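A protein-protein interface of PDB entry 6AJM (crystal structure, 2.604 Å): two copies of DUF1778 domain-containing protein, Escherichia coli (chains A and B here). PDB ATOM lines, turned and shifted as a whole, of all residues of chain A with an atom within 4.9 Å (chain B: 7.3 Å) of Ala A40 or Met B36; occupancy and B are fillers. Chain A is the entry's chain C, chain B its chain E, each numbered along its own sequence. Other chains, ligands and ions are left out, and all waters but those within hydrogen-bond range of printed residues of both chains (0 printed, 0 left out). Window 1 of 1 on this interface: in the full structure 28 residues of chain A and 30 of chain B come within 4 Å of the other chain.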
ATOM      1  N   ILE A   9      26.557  29.723  15.966  1.00  0.00           N
ATOM      2  CA  ILE A   9      27.824  30.296  16.410  1.00  0.00           C
ATOM      3  C   ILE A   9      28.942  29.358  15.955  1.00  0.00           C
ATOM      4  O   ILE A   9      28.909  28.159  16.248  1.00  0.00           O
ATOM      5  CB  ILE A   9      27.869  30.474  17.942  1.00  0.00           C
ATOM      6  CG1 ILE A   9      26.688  31.319  18.427  1.00  0.00           C
ATOM      7  CG2 ILE A   9      29.165  31.115  18.363  1.00  0.00           C
ATOM      8  CD1 ILE A   9      26.538  31.360  19.937  1.00  0.00           C
ATOM      9  N   LEU A  11      32.588  28.484  16.641  1.00  0.00           N
ATOM     10  CA  LEU A  11      33.723  28.618  17.542  1.00  0.00           C
ATOM     11  C   LEU A  11      34.970  28.064  16.862  1.00  0.00           C
ATOM     12  O   LEU A  11      34.934  26.981  16.266  1.00  0.00           O
ATOM     13  CB  LEU A  11      33.459  27.893  18.866  1.00  0.00           C
ATOM     14  CG  LEU A  11      32.292  28.477  19.656  1.00  0.00           C
ATOM     15  CD1 LEU A  11      32.271  27.965  21.077  1.00  0.00           C
ATOM     16  CD2 LEU A  11      32.366  29.979  19.649  1.00  0.00           C
ATOM     17  N   MET A  36      29.356  21.435  24.683  1.00  0.00           N
ATOM     18  CA  MET A  36      29.720  22.840  24.732  1.00  0.00           C
ATOM     19  C   MET A  36      28.502  23.709  24.986  1.00  0.00           C
ATOM     20  O   MET A  36      28.559  24.640  25.797  1.00  0.00           O
ATOM     21  CB  MET A  36      30.437  23.240  23.446  1.00  0.00           C
ATOM     22  CG  MET A  36      31.765  22.507  23.299  1.00  0.00           C
ATOM     23  SD  MET A  36      32.754  23.059  21.911  1.00  0.00           S
ATOM     24  CE  MET A  36      33.172  24.700  22.491  1.00  0.00           C
ATOM     25  N   LEU A  37      27.378  23.408  24.330  1.00  0.00           N
ATOM     26  CA  LEU A  37      26.200  24.254  24.491  1.00  0.00           C
ATOM     27  C   LEU A  37      25.587  24.099  25.879  1.00  0.00           C
ATOM     28  O   LEU A  37      25.108  25.077  26.465  1.00  0.00           O
ATOM     29  CB  LEU A  37      25.175  23.941  23.402  1.00  0.00           C
ATOM     30  CG  LEU A  37      23.751  24.480  23.593  1.00  0.00           C
ATOM     31  CD1 LEU A  37      23.714  25.995  23.785  1.00  0.00           C
ATOM     32  CD2 LEU A  37      22.866  24.052  22.425  1.00  0.00           C
ATOM     33  N   ASN A  38      25.627  22.886  26.442  1.00  0.00           N
ATOM     34  CA  ASN A  38      25.150  22.716  27.811  1.00  0.00           C
ATOM     35  C   ASN A  38      26.058  23.441  28.793  1.00  0.00           C
ATOM     36  O   ASN A  38      25.570  24.081  29.735  1.00  0.00           O
ATOM     37  CB  ASN A  38      25.032  21.227  28.158  1.00  0.00           C
ATOM     38  CG  ASN A  38      23.806  20.582  27.544  1.00  0.00           C
ATOM     39  OD1 ASN A  38      22.807  21.262  27.274  1.00  0.00           O
ATOM     40  ND2 ASN A  38      23.872  19.273  27.312  1.00  0.00           N
ATOM     41  N   SER A  39      27.379  23.389  28.560  1.00  0.00           N
ATOM     42  CA  SER A  39      28.324  24.094  29.421  1.00  0.00           C
ATOM     43  C   SER A  39      28.094  25.599  29.386  1.00  0.00           C
ATOM     44  O   SER A  39      28.009  26.257  30.434  1.00  0.00           O
ATOM     45  CB  SER A  39      29.753  23.758  29.005  1.00  0.00           C
ATOM     46  OG  SER A  39      30.042  22.394  29.255  1.00  0.00           O
ATOM     47  N   ALA A  40      27.957  26.162  28.186  1.00  0.00           N
ATOM     48  CA  ALA A  40      27.705  27.596  28.074  1.00  0.00           C
ATOM     49  C   ALA A  40      26.367  27.986  28.695  1.00  0.00           C
ATOM     50  O   ALA A  40      26.284  28.996  29.402  1.00  0.00           O
ATOM     51  CB  ALA A  40      27.756  28.033  26.612  1.00  0.00           C
ATOM     52  N   SER A  41      25.316  27.199  28.470  1.00  0.00           N
ATOM     53  CA  SER A  41      23.990  27.624  28.907  1.00  0.00           C
ATOM     54  C   SER A  41      23.857  27.575  30.423  1.00  0.00           C
ATOM     55  O   SER A  41      23.296  28.498  31.031  1.00  0.00           O
ATOM     56  CB  SER A  41      22.918  26.765  28.252  1.00  0.00           C
ATOM     57  OG  SER A  41      21.639  27.235  28.614  1.00  0.00           O
ATOM     58  N   GLN A  42      24.411  26.532  31.053  1.00  0.00           N
ATOM     59  CA  GLN A  42      24.389  26.450  32.511  1.00  0.00           C
ATOM     60  C   GLN A  42      25.299  27.503  33.144  1.00  0.00           C
ATOM     61  O   GLN A  42      24.925  28.130  34.148  1.00  0.00           O
ATOM     62  CB  GLN A  42      24.777  25.034  32.953  1.00  0.00           C
ATOM     63  CG  GLN A  42      23.874  23.949  32.322  1.00  0.00           C
ATOM     64  CD  GLN A  42      24.343  22.514  32.590  1.00  0.00           C
ATOM     65  OE1 GLN A  42      25.321  22.282  33.314  1.00  0.00           O
ATOM     66  NE2 GLN A  42      23.651  21.550  31.990  1.00  0.00           N
ATOM     67  N   ARG A  43      26.488  27.740  32.568  1.00  0.00           N
ATOM     68  CA  ARG A  43      27.375  28.742  33.158  1.00  0.00           C
ATOM     69  C   ARG A  43      26.775  30.135  33.048  1.00  0.00           C
ATOM     70  O   ARG A  43      26.869  30.926  33.993  1.00  0.00           O
ATOM     71  CB  ARG A  43      28.764  28.709  32.511  1.00  0.00           C
ATOM     72  CG  ARG A  43      29.780  29.660  33.176  1.00  0.00           C
ATOM     73  CD  ARG A  43      29.928  29.407  34.674  1.00  0.00           C
ATOM     74  NE  ARG A  43      30.994  30.197  35.295  1.00  0.00           N
ATOM     75  CZ  ARG A  43      30.939  30.663  36.541  1.00  0.00           C
ATOM     76  NH1 ARG A  43      29.871  30.432  37.294  1.00  0.00           N
ATOM     77  NH2 ARG A  43      31.939  31.371  37.038  1.00  0.00           N
ATOM     78  N   ALA A  44      26.162  30.455  31.903  1.00  0.00           N
ATOM     79  CA  ALA A  44      25.533  31.760  31.747  1.00  0.00           C
ATOM     80  C   ALA A  44      24.394  31.942  32.741  1.00  0.00           C
ATOM     81  O   ALA A  44      24.262  33.013  33.351  1.00  0.00           O
ATOM     82  CB  ALA A  44      25.034  31.932  30.316  1.00  0.00           C
ATOM     83  N   ALA A  45      23.568  30.903  32.927  1.00  0.00           N
ATOM     84  CA  ALA A  45      22.523  30.993  33.942  1.00  0.00           C
ATOM     85  C   ALA A  45      23.107  31.288  35.324  1.00  0.00           C
ATOM     86  O   ALA A  45      22.608  32.165  36.043  1.00  0.00           O
ATOM     87  CB  ALA A  45      21.694  29.714  33.958  1.00  0.00           C
ATOM     88  N   LEU B  11      27.700  25.230  16.270  1.00  0.00           N
ATOM     89  CA  LEU B  11      26.832  25.230  17.442  1.00  0.00           C
ATOM     90  C   LEU B  11      25.541  25.968  17.132  1.00  0.00           C
ATOM     91  O   LEU B  11      25.569  27.135  16.732  1.00  0.00           O
ATOM     92  CB  LEU B  11      27.517  25.871  18.650  1.00  0.00           C
ATOM     93  CG  LEU B  11      28.607  25.035  19.310  1.00  0.00           C
ATOM     94  CD1 LEU B  11      29.204  25.783  20.478  1.00  0.00           C
ATOM     95  CD2 LEU B  11      28.014  23.731  19.763  1.00  0.00           C
ATOM     96  N   LEU B  13      21.737  27.209  18.603  1.00  0.00           N
ATOM     97  CA  LEU B  13      20.953  27.493  19.809  1.00  0.00           C
ATOM     98  C   LEU B  13      19.592  28.136  19.515  1.00  0.00           C
ATOM     99  O   LEU B  13      19.157  28.160  18.362  1.00  0.00           O
ATOM    100  CB  LEU B  13      21.726  28.371  20.796  1.00  0.00           C
ATOM    101  CG  LEU B  13      23.137  28.918  20.679  1.00  0.00           C
ATOM    102  CD1 LEU B  13      23.385  29.708  19.408  1.00  0.00           C
ATOM    103  CD2 LEU B  13      23.313  29.820  21.866  1.00  0.00           C
ATOM    104  N   ASP B  17      18.807  30.704  24.615  1.00  0.00           N
ATOM    105  CA  ASP B  17      20.190  30.375  24.893  1.00  0.00           C
ATOM    106  C   ASP B  17      21.108  31.480  24.401  1.00  0.00           C
ATOM    107  O   ASP B  17      21.996  31.919  25.136  1.00  0.00           O
ATOM    108  CB  ASP B  17      20.542  29.019  24.264  1.00  0.00           C
ATOM    109  CG  ASP B  17      20.235  27.841  25.198  1.00  0.00           C
ATOM    110  OD1 ASP B  17      19.932  28.085  26.391  1.00  0.00           O
ATOM    111  OD2 ASP B  17      20.304  26.676  24.741  1.00  0.00           O
ATOM    112  N   LYS B  18      20.896  31.975  23.179  1.00  0.00           N
ATOM    113  CA  LYS B  18      21.837  32.959  22.653  1.00  0.00           C
ATOM    114  C   LYS B  18      21.766  34.266  23.433  1.00  0.00           C
ATOM    115  O   LYS B  18      22.797  34.828  23.819  1.00  0.00           O
ATOM    116  CB  LYS B  18      21.605  33.212  21.167  1.00  0.00           C
ATOM    117  CG  LYS B  18      22.619  34.187  20.625  1.00  0.00           C
ATOM    118  CD  LYS B  18      22.693  34.105  19.134  1.00  0.00           C
ATOM    119  CE  LYS B  18      23.843  34.947  18.605  1.00  0.00           C
ATOM    120  NZ  LYS B  18      23.877  34.942  17.114  1.00  0.00           N
ATOM    121  N   MET B  20      20.817  34.660  26.452  1.00  0.00           N
ATOM    122  CA  MET B  20      21.300  34.450  27.809  1.00  0.00           C
ATOM    123  C   MET B  20      22.816  34.364  27.848  1.00  0.00           C
ATOM    124  O   MET B  20      23.453  34.892  28.769  1.00  0.00           O
ATOM    125  CB  MET B  20      20.679  33.188  28.391  1.00  0.00           C
ATOM    126  CG  MET B  20      20.516  33.218  29.899  1.00  0.00           C
ATOM    127  SD  MET B  20      19.813  31.680  30.523  1.00  0.00           S
ATOM    128  CE  MET B  20      20.976  30.493  29.825  1.00  0.00           C
ATOM    129  N   ILE B  21      23.413  33.715  26.852  1.00  0.00           N
ATOM    130  CA  ILE B  21      24.863  33.690  26.746  1.00  0.00           C
ATOM    131  C   ILE B  21      25.410  35.093  26.500  1.00  0.00           C
ATOM    132  O   ILE B  21      26.418  35.481  27.094  1.00  0.00           O
ATOM    133  CB  ILE B  21      25.282  32.692  25.654  1.00  0.00           C
ATOM    134  CG1 ILE B  21      25.001  31.268  26.149  1.00  0.00           C
ATOM    135  CG2 ILE B  21      26.727  32.869  25.283  1.00  0.00           C
ATOM    136  CD1 ILE B  21      24.869  30.246  25.066  1.00  0.00           C
ATOM    137  N   ALA B  24      25.309  36.962  29.886  1.00  0.00           N
ATOM    138  CA  ALA B  24      26.363  36.527  30.801  1.00  0.00           C
ATOM    139  C   ALA B  24      27.736  36.957  30.321  1.00  0.00           C
ATOM    140  O   ALA B  24      28.600  37.316  31.133  1.00  0.00           O
ATOM    141  CB  ALA B  24      26.333  35.013  30.973  1.00  0.00           C
ATOM    142  N   ALA B  25      27.970  36.895  29.010  1.00  0.00           N
ATOM    143  CA  ALA B  25      29.249  37.330  28.461  1.00  0.00           C
ATOM    144  C   ALA B  25      29.471  38.816  28.700  1.00  0.00           C
ATOM    145  O   ALA B  25      30.583  39.236  29.047  1.00  0.00           O
ATOM    146  CB  ALA B  25      29.320  37.000  26.971  1.00  0.00           C
ATOM    147  N   GLN B  30      33.564  39.690  28.508  1.00  0.00           N
ATOM    148  CA  GLN B  30      34.143  38.765  27.541  1.00  0.00           C
ATOM    149  C   GLN B  30      33.364  38.815  26.240  1.00  0.00           C
ATOM    150  O   GLN B  30      32.209  39.239  26.204  1.00  0.00           O
ATOM    151  CB  GLN B  30      34.132  37.308  28.024  1.00  0.00           C
ATOM    152  CG  GLN B  30      35.048  36.989  29.177  1.00  0.00           C
ATOM    153  CD  GLN B  30      34.877  35.557  29.671  1.00  0.00           C
ATOM    154  OE1 GLN B  30      34.794  34.617  28.881  1.00  0.00           O
ATOM    155  NE2 GLN B  30      34.815  35.394  30.984  1.00  0.00           N
ATOM    156  N   SER B  31      34.011  38.353  25.173  1.00  0.00           N
ATOM    157  CA  SER B  31      33.312  38.077  23.933  1.00  0.00           C
ATOM    158  C   SER B  31      32.354  36.914  24.140  1.00  0.00           C
ATOM    159  O   SER B  31      32.437  36.172  25.124  1.00  0.00           O
ATOM    160  CB  SER B  31      34.303  37.748  22.817  1.00  0.00           C
ATOM    161  OG  SER B  31      33.660  37.161  21.700  1.00  0.00           O
ATOM    162  N   VAL B  32      31.428  36.758  23.198  1.00  0.00           N
ATOM    163  CA  VAL B  32      30.537  35.604  23.264  1.00  0.00           C
ATOM    164  C   VAL B  32      31.319  34.316  22.989  1.00  0.00           C
ATOM    165  O   VAL B  32      31.048  33.272  23.599  1.00  0.00           O
ATOM    166  CB  VAL B  32      29.332  35.832  22.317  1.00  0.00           C
ATOM    167  CG1 VAL B  32      28.695  34.537  21.859  1.00  0.00           C
ATOM    168  CG2 VAL B  32      28.274  36.691  23.020  1.00  0.00           C
ATOM    169  N   SER B  33      32.346  34.384  22.142  1.00  0.00           N
ATOM    170  CA  SER B  33      33.199  33.226  21.894  1.00  0.00           C
ATOM    171  C   SER B  33      34.085  32.920  23.091  1.00  0.00           C
ATOM    172  O   SER B  33      34.268  31.752  23.449  1.00  0.00           O
ATOM    173  CB  SER B  33      34.073  33.464  20.664  1.00  0.00           C
ATOM    174  OG  SER B  33      33.332  33.332  19.471  1.00  0.00           O
ATOM    175  N   GLN B  34      34.707  33.950  23.680  1.00  0.00           N
ATOM    176  CA  GLN B  34      35.503  33.714  24.878  1.00  0.00           C
ATOM    177  C   GLN B  34      34.662  33.036  25.948  1.00  0.00           C
ATOM    178  O   GLN B  34      35.125  32.100  26.606  1.00  0.00           O
ATOM    179  CB  GLN B  34      36.079  35.019  25.420  1.00  0.00           C
ATOM    180  CG  GLN B  34      36.795  35.868  24.414  1.00  0.00           C
ATOM    181  CD  GLN B  34      37.219  37.188  25.018  1.00  0.00           C
ATOM    182  OE1 GLN B  34      37.165  37.361  26.238  1.00  0.00           O
ATOM    183  NE2 GLN B  34      37.633  38.132  24.172  1.00  0.00           N
ATOM    184  N   PHE B  35      33.406  33.485  26.112  1.00  0.00           N
ATOM    185  CA  PHE B  35      32.524  32.940  27.142  1.00  0.00           C
ATOM    186  C   PHE B  35      32.158  31.492  26.850  1.00  0.00           C
ATOM    187  O   PHE B  35      32.201  30.631  27.741  1.00  0.00           O
ATOM    188  CB  PHE B  35      31.249  33.773  27.254  1.00  0.00           C
ATOM    189  CG  PHE B  35      30.395  33.390  28.423  1.00  0.00           C
ATOM    190  CD1 PHE B  35      30.484  34.087  29.624  1.00  0.00           C
ATOM    191  CD2 PHE B  35      29.529  32.324  28.339  1.00  0.00           C
ATOM    192  CE1 PHE B  35      29.720  33.734  30.714  1.00  0.00           C
ATOM    193  CE2 PHE B  35      28.767  31.964  29.430  1.00  0.00           C
ATOM    194  CZ  PHE B  35      28.864  32.671  30.619  1.00  0.00           C
ATOM    195  N   MET B  36      31.775  31.203  25.608  1.00  0.00           N
ATOM    196  CA  MET B  36      31.451  29.825  25.279  1.00  0.00           C
ATOM    197  C   MET B  36      32.663  28.914  25.465  1.00  0.00           C
ATOM    198  O   MET B  36      32.547  27.841  26.075  1.00  0.00           O
ATOM    199  CB  MET B  36      30.871  29.758  23.867  1.00  0.00           C
ATOM    200  CG  MET B  36      29.515  30.460  23.839  1.00  0.00           C
ATOM    201  SD  MET B  36      28.341  29.888  22.593  1.00  0.00           S
ATOM    202  CE  MET B  36      28.204  28.160  23.022  1.00  0.00           C
ATOM    203  N   LEU B  37      33.846  29.351  25.011  1.00  0.00           N
ATOM    204  CA  LEU B  37      35.044  28.522  25.132  1.00  0.00           C
ATOM    205  C   LEU B  37      35.440  28.325  26.587  1.00  0.00           C
ATOM    206  O   LEU B  37      35.731  27.204  27.008  1.00  0.00           O
ATOM    207  CB  LEU B  37      36.202  29.136  24.345  1.00  0.00           C
ATOM    208  CG  LEU B  37      36.031  28.971  22.836  1.00  0.00           C
ATOM    209  CD1 LEU B  37      37.183  29.577  22.045  1.00  0.00           C
ATOM    210  CD2 LEU B  37      35.885  27.505  22.529  1.00  0.00           C
ATOM    211  N   ASN B  38      35.483  29.405  27.370  1.00  0.00           N
ATOM    212  CA  ASN B  38      35.857  29.279  28.770  1.00  0.00           C
ATOM    213  C   ASN B  38      34.871  28.401  29.528  1.00  0.00           C
ATOM    214  O   ASN B  38      35.284  27.577  30.354  1.00  0.00           O
ATOM    215  CB  ASN B  38      35.975  30.661  29.404  1.00  0.00           C
ATOM    216  CG  ASN B  38      37.225  31.387  28.965  1.00  0.00           C
ATOM    217  OD1 ASN B  38      38.290  30.784  28.844  1.00  0.00           O
ATOM    218  ND2 ASN B  38      37.101  32.684  28.710  1.00  0.00           N
ATOM    219  N   SER B  39      33.570  28.538  29.243  1.00  0.00           N
ATOM    220  CA  SER B  39      32.578  27.685  29.895  1.00  0.00           C
ATOM    221  C   SER B  39      32.819  26.217  29.577  1.00  0.00           C
ATOM    222  O   SER B  39      32.900  25.383  30.486  1.00  0.00           O
ATOM    223  CB  SER B  39      31.171  28.093  29.469  1.00  0.00           C
ATOM    224  OG  SER B  39      30.838  29.352  30.010  1.00  0.00           O
ATOM    225  N   ALA B  40      32.940  25.888  28.286  1.00  0.00           N
ATOM    226  CA  ALA B  40      33.217  24.511  27.887  1.00  0.00           C
ATOM    227  C   ALA B  40      34.530  24.006  28.483  1.00  0.00           C
ATOM    228  O   ALA B  40      34.614  22.858  28.929  1.00  0.00           O
ATOM    229  CB  ALA B  40      33.244  24.406  26.361  1.00  0.00           C
ATOM    230  N   SER B  41      35.553  24.859  28.522  1.00  0.00           N
ATOM    231  CA  SER B  41      36.876  24.446  28.972  1.00  0.00           C
ATOM    232  C   SER B  41      36.887  24.148  30.462  1.00  0.00           C
ATOM    233  O   SER B  41      37.357  23.084  30.889  1.00  0.00           O
ATOM    234  CB  SER B  41      37.886  25.533  28.640  1.00  0.00           C
ATOM    235  OG  SER B  41      38.638  25.163  27.505  1.00  0.00           O
ATOM    236  N   GLN B  42      36.364  25.076  31.271  1.00  0.00           N
ATOM    237  CA  GLN B  42      36.274  24.830  32.704  1.00  0.00           C
ATOM    238  C   GLN B  42      35.377  23.635  33.007  1.00  0.00           C
ATOM    239  O   GLN B  42      35.706  22.819  33.874  1.00  0.00           O
ATOM    240  CB  GLN B  42      35.781  26.083  33.421  1.00  0.00           C
ATOM    241  CG  GLN B  42      36.662  27.274  33.180  1.00  0.00           C
ATOM    242  CD  GLN B  42      36.163  28.536  33.862  1.00  0.00           C
ATOM    243  OE1 GLN B  42      35.150  28.525  34.565  1.00  0.00           O
ATOM    244  NE2 GLN B  42      36.879  29.637  33.656  1.00  0.00           N
ATOM    245  N   ARG B  43      34.251  23.496  32.294  1.00  0.00           N
ATOM    246  CA  ARG B  43      33.377  22.363  32.557  1.00  0.00           C
ATOM    247  C   ARG B  43      34.056  21.046  32.208  1.00  0.00           C
ATOM    248  O   ARG B  43      33.961  20.074  32.967  1.00  0.00           O
ATOM    249  CB  ARG B  43      32.085  22.492  31.772  1.00  0.00           C
ATOM    250  CG  ARG B  43      30.997  21.588  32.274  1.00  0.00           C
ATOM    251  CD  ARG B  43      30.449  22.077  33.603  1.00  0.00           C
ATOM    252  NE  ARG B  43      29.075  21.622  33.768  1.00  0.00           N
ATOM    253  CZ  ARG B  43      28.743  20.494  34.382  1.00  0.00           C
ATOM    254  NH1 ARG B  43      29.694  19.726  34.907  1.00  0.00           N
ATOM    255  NH2 ARG B  43      27.466  20.145  34.485  1.00  0.00           N
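O of Leu B11 sits at hydrogen-bond distance from N of Ile A9, 2.9 Å away. The side-chain hydroxyl (OG) of Ser A41 sits at hydrogen-bond distance from the side-chain carboxylate (OD1) of Asp B17, 2.9 Å away. OE1 of Gln A42 is in hydrogen-bond range of NH2 of Arg B43, 3.2 Å away.
OE1 of Gln B30 sits at hydrogen-bond distance from N of Phe B35 (3.3 Å). The backbone NH (N) of Ser B33 sits at hydrogen-bond distance from the side-chain hydroxyl (OG) of Ser B31 (3.1 Å). O of Phe B35 lies within hydrogen-bond range of OG of Ser B39 (2.9 Å).
CD1 of Leu B13 touches CD1 of Ile A9, 3.6 Å away. OG of Ser B33 touches CD2 of Leu A11, 3.5 Å away. Leu A11 touches Met B36. Ala B40 touches Met A36 (CB to CE, 3.9 Å). OD2 of Asp B17 touches CD1 of Leu A37, 3.6 Å away. Ala B40 touches Ser A39. Arg B43 touches Ser A39. O of Ala A40 touches CE2 of Phe B35, 3.9 Å away. O of Ser A41 touches CE of Met B20 (3.3 Å). CB of Ala A44 touches CA of Ile B21 (3.98 Å).
Printed residues of chain B within 4 Å of Leu A37: Asp B17. Of chain B, only Ile B21 (3.95 Å), Phe B35 (3.9 Å), Met B36 (3.6 Å) and Ser B39 (3.8 Å) come within 4 Å of Ala A40. Of the printed residues of chain B, Ala A44 touches Met B20, Ile B21, Ala B24 and Phe B35. Printed residues of chain A within 4 Å of Ala B24: Ala A44. Ala B25 touches none of the printed residues of chain A. Of the printed residues of chain A, Ser B33 touches Leu A11. Of chain A, only Ile A9 (3.5 Å), Leu A11 (3.6 Å) and Ala A40 (3.6 Å) come within 4 Å of Met B36. The nearest residue of chain A that does not touch Met B36 is Met A36 (4.5 Å). The nearest printed residue of chain B that does not touch Leu A11 is Val B32 (5.3 Å).
Of the 12 printed residues of chain A, 10 touch a printed residue of chain B. Printed residues of chain A that touch a printed residue of chain B: Ile A9, Leu A11, Met A36, Leu A37, Ser A39, Ala A40, Ser A41, Gln A42, Arg A43 and Ala A44. Printed residues of chain B that touch a printed residue of chain A: Leu B11, Leu B13, Asp B17, Met B20, Ile B21, Ala B24, Ser B33, Phe B35, Met B36, Leu B37, Ser B39, Ala B40 and Arg B43. Among the printed residues, no Asp or Glu carboxylate lies within 4 Å of a Lys or Arg side-chain nitrogen of the other chain.
Leu A11 touches Met B36, but with the chains exchanged Met A36 does not touch Leu B11 (4.1 Å). Leu A11 touches Leu B37, but with the chains exchanged Leu A37 does not touch Leu B11 (4.6 Å). Met A36 touches Leu B37, but with the chains exchanged Leu A37 does not touch Met B36 (4.6 Å). Ser A39 touches Arg B43, and with the chains exchanged Arg A43 touches Ser B39. Positions printed for both chains: 11, 36, 37, 38, 39, 40, 41, 42 and 43.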
